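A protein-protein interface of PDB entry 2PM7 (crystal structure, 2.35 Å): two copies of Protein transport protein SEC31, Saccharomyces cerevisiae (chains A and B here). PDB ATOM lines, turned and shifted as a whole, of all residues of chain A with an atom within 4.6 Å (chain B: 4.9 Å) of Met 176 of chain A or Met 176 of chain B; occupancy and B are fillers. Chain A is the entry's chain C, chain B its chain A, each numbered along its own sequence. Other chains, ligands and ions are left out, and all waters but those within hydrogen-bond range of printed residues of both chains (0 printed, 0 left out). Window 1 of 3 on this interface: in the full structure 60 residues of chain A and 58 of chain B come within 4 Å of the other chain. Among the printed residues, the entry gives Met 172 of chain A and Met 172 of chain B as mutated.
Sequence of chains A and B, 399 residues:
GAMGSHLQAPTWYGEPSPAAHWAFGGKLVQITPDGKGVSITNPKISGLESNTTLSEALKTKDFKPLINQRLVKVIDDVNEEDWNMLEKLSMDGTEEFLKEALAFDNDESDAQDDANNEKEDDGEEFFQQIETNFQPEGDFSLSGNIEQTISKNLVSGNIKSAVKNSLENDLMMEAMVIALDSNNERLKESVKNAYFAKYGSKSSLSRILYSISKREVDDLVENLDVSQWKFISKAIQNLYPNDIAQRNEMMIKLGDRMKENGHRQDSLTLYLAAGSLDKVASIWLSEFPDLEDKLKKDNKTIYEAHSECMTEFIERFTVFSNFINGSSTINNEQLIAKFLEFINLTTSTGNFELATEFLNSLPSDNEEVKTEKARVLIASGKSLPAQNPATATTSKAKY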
ATOM      1  N   MET A 172      34.911  -6.259 -12.550  1.00  0.00           N
ATOM      2  CA  MET A 172      33.515  -6.423 -12.176  1.00  0.00           C
ATOM      3  C   MET A 172      33.128  -7.746 -11.514  1.00  0.00           C
ATOM      4  O   MET A 172      32.469  -7.731 -10.481  1.00  0.00           O
ATOM      5  CB  MET A 172      32.623  -6.157 -13.378  1.00  0.00           C
ATOM      6  CG  MET A 172      31.196  -5.922 -12.983  1.00  0.00           C
ATOM      7  SD  MET A 172      30.381  -4.788 -14.250  1.00  0.00           S
ATOM      8  CE  MET A 172      30.495  -3.123 -13.278  1.00  0.00           C
ATOM      9  N   MET A 173      33.515  -8.882 -12.093  1.00  0.00           N
ATOM     10  CA  MET A 173      33.189 -10.164 -11.474  1.00  0.00           C
ATOM     11  C   MET A 173      33.670 -10.149 -10.033  1.00  0.00           C
ATOM     12  O   MET A 173      33.017 -10.692  -9.141  1.00  0.00           O
ATOM     13  CB  MET A 173      33.861 -11.331 -12.201  1.00  0.00           C
ATOM     14  CG  MET A 173      33.250 -11.661 -13.540  1.00  0.00           C
ATOM     15  SD  MET A 173      33.867 -13.356 -14.194  1.00  0.00           S
ATOM     16  CE  MET A 173      35.670 -12.842 -14.697  1.00  0.00           C
ATOM     17  N   GLU A 174      34.822  -9.520  -9.820  1.00  0.00           N
ATOM     18  CA  GLU A 174      35.412  -9.417  -8.496  1.00  0.00           C
ATOM     19  C   GLU A 174      34.442  -8.677  -7.584  1.00  0.00           C
ATOM     20  O   GLU A 174      34.102  -9.154  -6.506  1.00  0.00           O
ATOM     21  CB  GLU A 174      36.734  -8.648  -8.570  1.00  0.00           C
ATOM     22  CG  GLU A 174      37.476  -8.778  -9.900  1.00  0.00           C
ATOM     23  CD  GLU A 174      37.951 -10.180 -10.185  1.00  0.00           C
ATOM     24  OE1 GLU A 174      37.101 -11.067 -10.378  1.00  0.00           O
ATOM     25  OE2 GLU A 174      39.180 -10.395 -10.216  1.00  0.00           O
ATOM     26  N   ALA A 175      33.997  -7.509  -8.028  1.00  0.00           N
ATOM     27  CA  ALA A 175      33.065  -6.697  -7.255  1.00  0.00           C
ATOM     28  C   ALA A 175      31.799  -7.490  -6.955  1.00  0.00           C
ATOM     29  O   ALA A 175      31.259  -7.420  -5.852  1.00  0.00           O
ATOM     30  CB  ALA A 175      32.717  -5.429  -8.026  1.00  0.00           C
ATOM     31  N   MET A 176      31.334  -8.242  -7.947  1.00  0.00           N
ATOM     32  CA  MET A 176      30.131  -9.046  -7.791  1.00  0.00           C
ATOM     33  C   MET A 176      30.346 -10.145  -6.765  1.00  0.00           C
ATOM     34  O   MET A 176      29.670 -10.178  -5.740  1.00  0.00           O
ATOM     35  CB  MET A 176      29.708  -9.650  -9.135  1.00  0.00           C
ATOM     36  CG  MET A 176      29.035  -8.650 -10.074  1.00  0.00           C
ATOM     37  SD  MET A 176      28.793  -9.346 -11.857  1.00  0.00           S
ATOM     38  CE  MET A 176      28.250  -7.740 -12.754  1.00  0.00           C
ATOM     39  N   VAL A 177      31.293 -11.035  -7.037  1.00  0.00           N
ATOM     40  CA  VAL A 177      31.588 -12.132  -6.124  1.00  0.00           C
ATOM     41  C   VAL A 177      31.672 -11.638  -4.683  1.00  0.00           C
ATOM     42  O   VAL A 177      31.291 -12.348  -3.757  1.00  0.00           O
ATOM     43  CB  VAL A 177      32.916 -12.824  -6.487  1.00  0.00           C
ATOM     44  CG1 VAL A 177      33.254 -13.869  -5.451  1.00  0.00           C
ATOM     45  CG2 VAL A 177      32.812 -13.466  -7.858  1.00  0.00           C
ATOM     46  N   ILE A 178      32.166 -10.418  -4.497  1.00  0.00           N
ATOM     47  CA  ILE A 178      32.283  -9.846  -3.161  1.00  0.00           C
ATOM     48  C   ILE A 178      30.919  -9.429  -2.631  1.00  0.00           C
ATOM     49  O   ILE A 178      30.490  -9.906  -1.587  1.00  0.00           O
ATOM     50  CB  ILE A 178      33.232  -8.617  -3.151  1.00  0.00           C
ATOM     51  CG1 ILE A 178      34.684  -9.081  -3.239  1.00  0.00           C
ATOM     52  CG2 ILE A 178      33.026  -7.795  -1.887  1.00  0.00           C
ATOM     53  CD1 ILE A 178      35.671  -7.945  -3.383  1.00  0.00           C
ATOM     54  N   ALA A 179      30.241  -8.538  -3.349  1.00  0.00           N
ATOM     55  CA  ALA A 179      28.922  -8.060  -2.934  1.00  0.00           C
ATOM     56  C   ALA A 179      27.936  -9.225  -2.840  1.00  0.00           C
ATOM     57  O   ALA A 179      26.988  -9.199  -2.055  1.00  0.00           O
ATOM     58  CB  ALA A 179      28.411  -7.014  -3.921  1.00  0.00           C
ATOM     59  N   LEU A 180      28.175 -10.247  -3.649  1.00  0.00           N
ATOM     60  CA  LEU A 180      27.339 -11.434  -3.672  1.00  0.00           C
ATOM     61  C   LEU A 180      27.613 -12.255  -2.420  1.00  0.00           C
ATOM     62  O   LEU A 180      27.079 -13.352  -2.255  1.00  0.00           O
ATOM     63  CB  LEU A 180      27.664 -12.262  -4.915  1.00  0.00           C
ATOM     64  CG  LEU A 180      26.836 -13.512  -5.192  1.00  0.00           C
ATOM     65  CD1 LEU A 180      25.378 -13.129  -5.362  1.00  0.00           C
ATOM     66  CD2 LEU A 180      27.354 -14.189  -6.444  1.00  0.00           C
ATOM     67  N   VAL A 191      26.619  -2.403  -7.360  1.00  0.00           N
ATOM     68  CA  VAL A 191      27.299  -3.296  -8.274  1.00  0.00           C
ATOM     69  C   VAL A 191      26.417  -3.597  -9.468  1.00  0.00           C
ATOM     70  O   VAL A 191      26.890  -3.631 -10.605  1.00  0.00           O
ATOM     71  CB  VAL A 191      27.647  -4.620  -7.578  1.00  0.00           C
ATOM     72  CG1 VAL A 191      28.371  -5.546  -8.540  1.00  0.00           C
ATOM     73  CG2 VAL A 191      28.499  -4.344  -6.351  1.00  0.00           C
ATOM     74  N   TYR A 195      27.016  -2.720 -13.438  1.00  0.00           N
ATOM     75  CA  TYR A 195      26.926  -3.714 -14.500  1.00  0.00           C
ATOM     76  C   TYR A 195      26.074  -3.206 -15.660  1.00  0.00           C
ATOM     77  O   TYR A 195      26.498  -3.214 -16.816  1.00  0.00           O
ATOM     78  CB  TYR A 195      26.314  -5.006 -13.955  1.00  0.00           C
ATOM     79  CG  TYR A 195      25.927  -5.989 -15.032  1.00  0.00           C
ATOM     80  CD1 TYR A 195      26.888  -6.764 -15.681  1.00  0.00           C
ATOM     81  CD2 TYR A 195      24.597  -6.127 -15.426  1.00  0.00           C
ATOM     82  CE1 TYR A 195      26.529  -7.657 -16.698  1.00  0.00           C
ATOM     83  CE2 TYR A 195      24.228  -7.011 -16.441  1.00  0.00           C
ATOM     84  CZ  TYR A 195      25.197  -7.772 -17.072  1.00  0.00           C
ATOM     85  OH  TYR A 195      24.832  -8.636 -18.079  1.00  0.00           O
ATOM     86  N   MET B 172      28.570 -15.850 -17.134  1.00  0.00           N
ATOM     87  CA  MET B 172      28.684 -15.895 -15.683  1.00  0.00           C
ATOM     88  C   MET B 172      28.379 -14.575 -14.989  1.00  0.00           C
ATOM     89  O   MET B 172      27.845 -14.572 -13.880  1.00  0.00           O
ATOM     90  CB  MET B 172      30.077 -16.372 -15.284  1.00  0.00           C
ATOM     91  CG  MET B 172      30.243 -16.596 -13.795  1.00  0.00           C
ATOM     92  SD  MET B 172      31.906 -17.455 -13.433  1.00  0.00           S
ATOM     93  CE  MET B 172      31.319 -19.286 -13.599  1.00  0.00           C
ATOM     94  N   MET B 173      28.729 -13.456 -15.619  1.00  0.00           N
ATOM     95  CA  MET B 173      28.436 -12.161 -15.015  1.00  0.00           C
ATOM     96  C   MET B 173      26.928 -12.039 -14.827  1.00  0.00           C
ATOM     97  O   MET B 173      26.451 -11.493 -13.834  1.00  0.00           O
ATOM     98  CB  MET B 173      28.914 -11.014 -15.901  1.00  0.00           C
ATOM     99  CG  MET B 173      30.259 -10.440 -15.523  1.00  0.00           C
ATOM    100  SD  MET B 173      30.437  -8.683 -16.275  1.00  0.00           S
ATOM    101  CE  MET B 173      30.735  -9.205 -18.103  1.00  0.00           C
ATOM    102  N   GLU B 174      26.184 -12.550 -15.799  1.00  0.00           N
ATOM    103  CA  GLU B 174      24.735 -12.500 -15.747  1.00  0.00           C
ATOM    104  C   GLU B 174      24.253 -13.458 -14.655  1.00  0.00           C
ATOM    105  O   GLU B 174      23.396 -13.105 -13.839  1.00  0.00           O
ATOM    106  CB  GLU B 174      24.160 -12.869 -17.121  1.00  0.00           C
ATOM    107  CG  GLU B 174      24.599 -11.913 -18.245  1.00  0.00           C
ATOM    108  CD  GLU B 174      25.970 -12.255 -18.845  1.00  0.00           C
ATOM    109  OE1 GLU B 174      26.894 -12.649 -18.101  1.00  0.00           O
ATOM    110  OE2 GLU B 174      26.124 -12.114 -20.077  1.00  0.00           O
ATOM    111  N   ALA B 175      24.826 -14.659 -14.637  1.00  0.00           N
ATOM    112  CA  ALA B 175      24.493 -15.659 -13.632  1.00  0.00           C
ATOM    113  C   ALA B 175      24.602 -15.011 -12.260  1.00  0.00           C
ATOM    114  O   ALA B 175      23.753 -15.214 -11.392  1.00  0.00           O
ATOM    115  CB  ALA B 175      25.454 -16.830 -13.721  1.00  0.00           C
ATOM    116  N   MET B 176      25.657 -14.224 -12.076  1.00  0.00           N
ATOM    117  CA  MET B 176      25.894 -13.537 -10.813  1.00  0.00           C
ATOM    118  C   MET B 176      24.886 -12.424 -10.544  1.00  0.00           C
ATOM    119  O   MET B 176      24.393 -12.299  -9.429  1.00  0.00           O
ATOM    120  CB  MET B 176      27.312 -12.958 -10.788  1.00  0.00           C
ATOM    121  CG  MET B 176      28.410 -14.007 -10.802  1.00  0.00           C
ATOM    122  SD  MET B 176      30.189 -13.244 -10.717  1.00  0.00           S
ATOM    123  CE  MET B 176      30.768 -13.615 -12.508  1.00  0.00           C
ATOM    124  N   VAL B 177      24.591 -11.614 -11.559  1.00  0.00           N
ATOM    125  CA  VAL B 177      23.642 -10.510 -11.412  1.00  0.00           C
ATOM    126  C   VAL B 177      22.262 -11.037 -11.052  1.00  0.00           C
ATOM    127  O   VAL B 177      21.568 -10.467 -10.216  1.00  0.00           O
ATOM    128  CB  VAL B 177      23.526  -9.674 -12.709  1.00  0.00           C
ATOM    129  CG1 VAL B 177      22.378  -8.687 -12.586  1.00  0.00           C
ATOM    130  CG2 VAL B 177      24.825  -8.924 -12.967  1.00  0.00           C
ATOM    131  N   ILE B 178      21.858 -12.118 -11.703  1.00  0.00           N
ATOM    132  CA  ILE B 178      20.567 -12.713 -11.410  1.00  0.00           C
ATOM    133  C   ILE B 178      20.637 -13.183  -9.960  1.00  0.00           C
ATOM    134  O   ILE B 178      19.778 -12.857  -9.142  1.00  0.00           O
ATOM    135  CB  ILE B 178      20.301 -13.935 -12.307  1.00  0.00           C
ATOM    136  CG1 ILE B 178      20.214 -13.505 -13.769  1.00  0.00           C
ATOM    137  CG2 ILE B 178      19.021 -14.622 -11.875  1.00  0.00           C
ATOM    138  CD1 ILE B 178      20.215 -14.665 -14.727  1.00  0.00           C
ATOM    139  N   ALA B 179      21.690 -13.939  -9.655  1.00  0.00           N
ATOM    140  CA  ALA B 179      21.903 -14.490  -8.321  1.00  0.00           C
ATOM    141  C   ALA B 179      22.074 -13.421  -7.244  1.00  0.00           C
ATOM    142  O   ALA B 179      21.906 -13.695  -6.058  1.00  0.00           O
ATOM    143  CB  ALA B 179      23.115 -15.413  -8.336  1.00  0.00           C
ATOM    144  N   LEU B 180      22.415 -12.209  -7.657  1.00  0.00           N
ATOM    145  CA  LEU B 180      22.600 -11.118  -6.713  1.00  0.00           C
ATOM    146  C   LEU B 180      21.245 -10.453  -6.512  1.00  0.00           C
ATOM    147  O   LEU B 180      21.130  -9.413  -5.854  1.00  0.00           O
ATOM    148  CB  LEU B 180      23.605 -10.109  -7.275  1.00  0.00           C
ATOM    149  CG  LEU B 180      24.053  -8.942  -6.391  1.00  0.00           C
ATOM    150  CD1 LEU B 180      24.811  -9.469  -5.183  1.00  0.00           C
ATOM    151  CD2 LEU B 180      24.939  -8.010  -7.200  1.00  0.00           C
ATOM    152  N   VAL B 191      26.880 -20.197  -7.688  1.00  0.00           N
ATOM    153  CA  VAL B 191      27.497 -19.283  -8.644  1.00  0.00           C
ATOM    154  C   VAL B 191      28.946 -19.002  -8.247  1.00  0.00           C
ATOM    155  O   VAL B 191      29.853 -19.117  -9.071  1.00  0.00           O
ATOM    156  CB  VAL B 191      26.730 -17.938  -8.705  1.00  0.00           C
ATOM    157  CG1 VAL B 191      27.406 -16.997  -9.677  1.00  0.00           C
ATOM    158  CG2 VAL B 191      25.293 -18.177  -9.116  1.00  0.00           C
ATOM    159  N   TYR B 195      32.513 -19.554 -10.093  1.00  0.00           N
ATOM    160  CA  TYR B 195      33.484 -18.496 -10.357  1.00  0.00           C
ATOM    161  C   TYR B 195      34.876 -19.011 -10.047  1.00  0.00           C
ATOM    162  O   TYR B 195      35.741 -19.086 -10.925  1.00  0.00           O
ATOM    163  CB  TYR B 195      33.207 -17.267  -9.484  1.00  0.00           C
ATOM    164  CG  TYR B 195      34.304 -16.220  -9.543  1.00  0.00           C
ATOM    165  CD1 TYR B 195      34.565 -15.516 -10.720  1.00  0.00           C
ATOM    166  CD2 TYR B 195      35.105 -15.956  -8.432  1.00  0.00           C
ATOM    167  CE1 TYR B 195      35.598 -14.576 -10.792  1.00  0.00           C
ATOM    168  CE2 TYR B 195      36.139 -15.019  -8.494  1.00  0.00           C
ATOM    169  CZ  TYR B 195      36.379 -14.336  -9.676  1.00  0.00           C
ATOM    170  OH  TYR B 195      37.402 -13.421  -9.747  1.00  0.00           O
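The side-chain hydroxyl (OH) of Tyr 195 of chain B lies within hydrogen-bond range of the side-chain carboxylate (OE1) of Glu 174 of chain A. The backbone carbonyl oxygen (O) of Met 173 of chain B sits close to the side-chain sulfur (SD) of Met 176 of chain A (3.7 Å).
Among the printed residues, pairs that only touch across the chains: Tyr 195 of chain A with Glu 174 of chain B (3.3 Å), Met 173 of chain A with Met 176 of chain B (3.3 Å), Val 177 of chain A with Tyr 195 of chain B (3.4 Å), Leu 180 of chain A with Leu 180 of chain B (3.5 Å), Leu 180 of chain A with Ala 179 of chain B (3.6 Å), Met 176 of chain A with Val 177 of chain B (3.6 Å), Tyr 195 of chain A with Val 177 of chain B (3.7 Å), Met 173 of chain A with Met 173 of chain B (3.8 Å), Ala 179 of chain A with Leu 180 of chain B (3.8 Å), Val 177 of chain A with Met 176 of chain B (3.9 Å), Met 173 of chain A with Tyr 195 of chain B (3.9 Å) and Met 176 of chain A with Met 176 of chain B (3.96 Å).
Of the printed residues of chain B, Met 176 of chain A touches Met 173, Met 176 and Val 177. Of chain A, only Met 173, Met 176 and Val 177 come within 4 Å of Met 176 of chain B. Printed residues of chain A within 4 Å of Leu 180 of chain B: Ala 179 and Leu 180. Printed residues of chain A within 4 Å of Met 173 of chain B: Met 173 and Met 176. Val 191 of chain A touches none of the printed residues of chain B. The nearest printed residue of chain B that does not touch Met 176 of chain A is Leu 180 of chain B (4.9 Å). The nearest residue of chain A that does not touch Met 176 of chain B is Leu 180 of chain A (4.3 Å).
Printed residues of chain A that touch a printed residue of chain B: Met 173, Glu 174, Met 176, Val 177, Ala 179, Leu 180 and Tyr 195. Of the 11 printed residues of chain B, 7 touch a printed residue of chain A. Hydrophobic or aromatic side chains of chain B within 4 Å of the printed part of chain A: Met 173, Met 176, Val 177, Leu 180 and Tyr 195. Among the printed residues, 14 pairs touch across the chains.
Met 173 of chain A touches Tyr 195 of chain B, but with the chains exchanged Tyr 195 of chain A does not touch Met 173 of chain B (4.1 Å). Glu 174 of chain A touches Tyr 195 of chain B, and with the chains exchanged Tyr 195 of chain A touches Glu 174 of chain B. Met 176 of chain A touches Val 177 of chain B, and with the chains exchanged Val 177 of chain A touches Met 176 of chain B. Leu 180 of chain B touches its own counterpart, Leu 180 of chain A. Of the 14 pairs that touch across the chains among the printed residues, 13 have their exchanged pair printed and touching as well.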
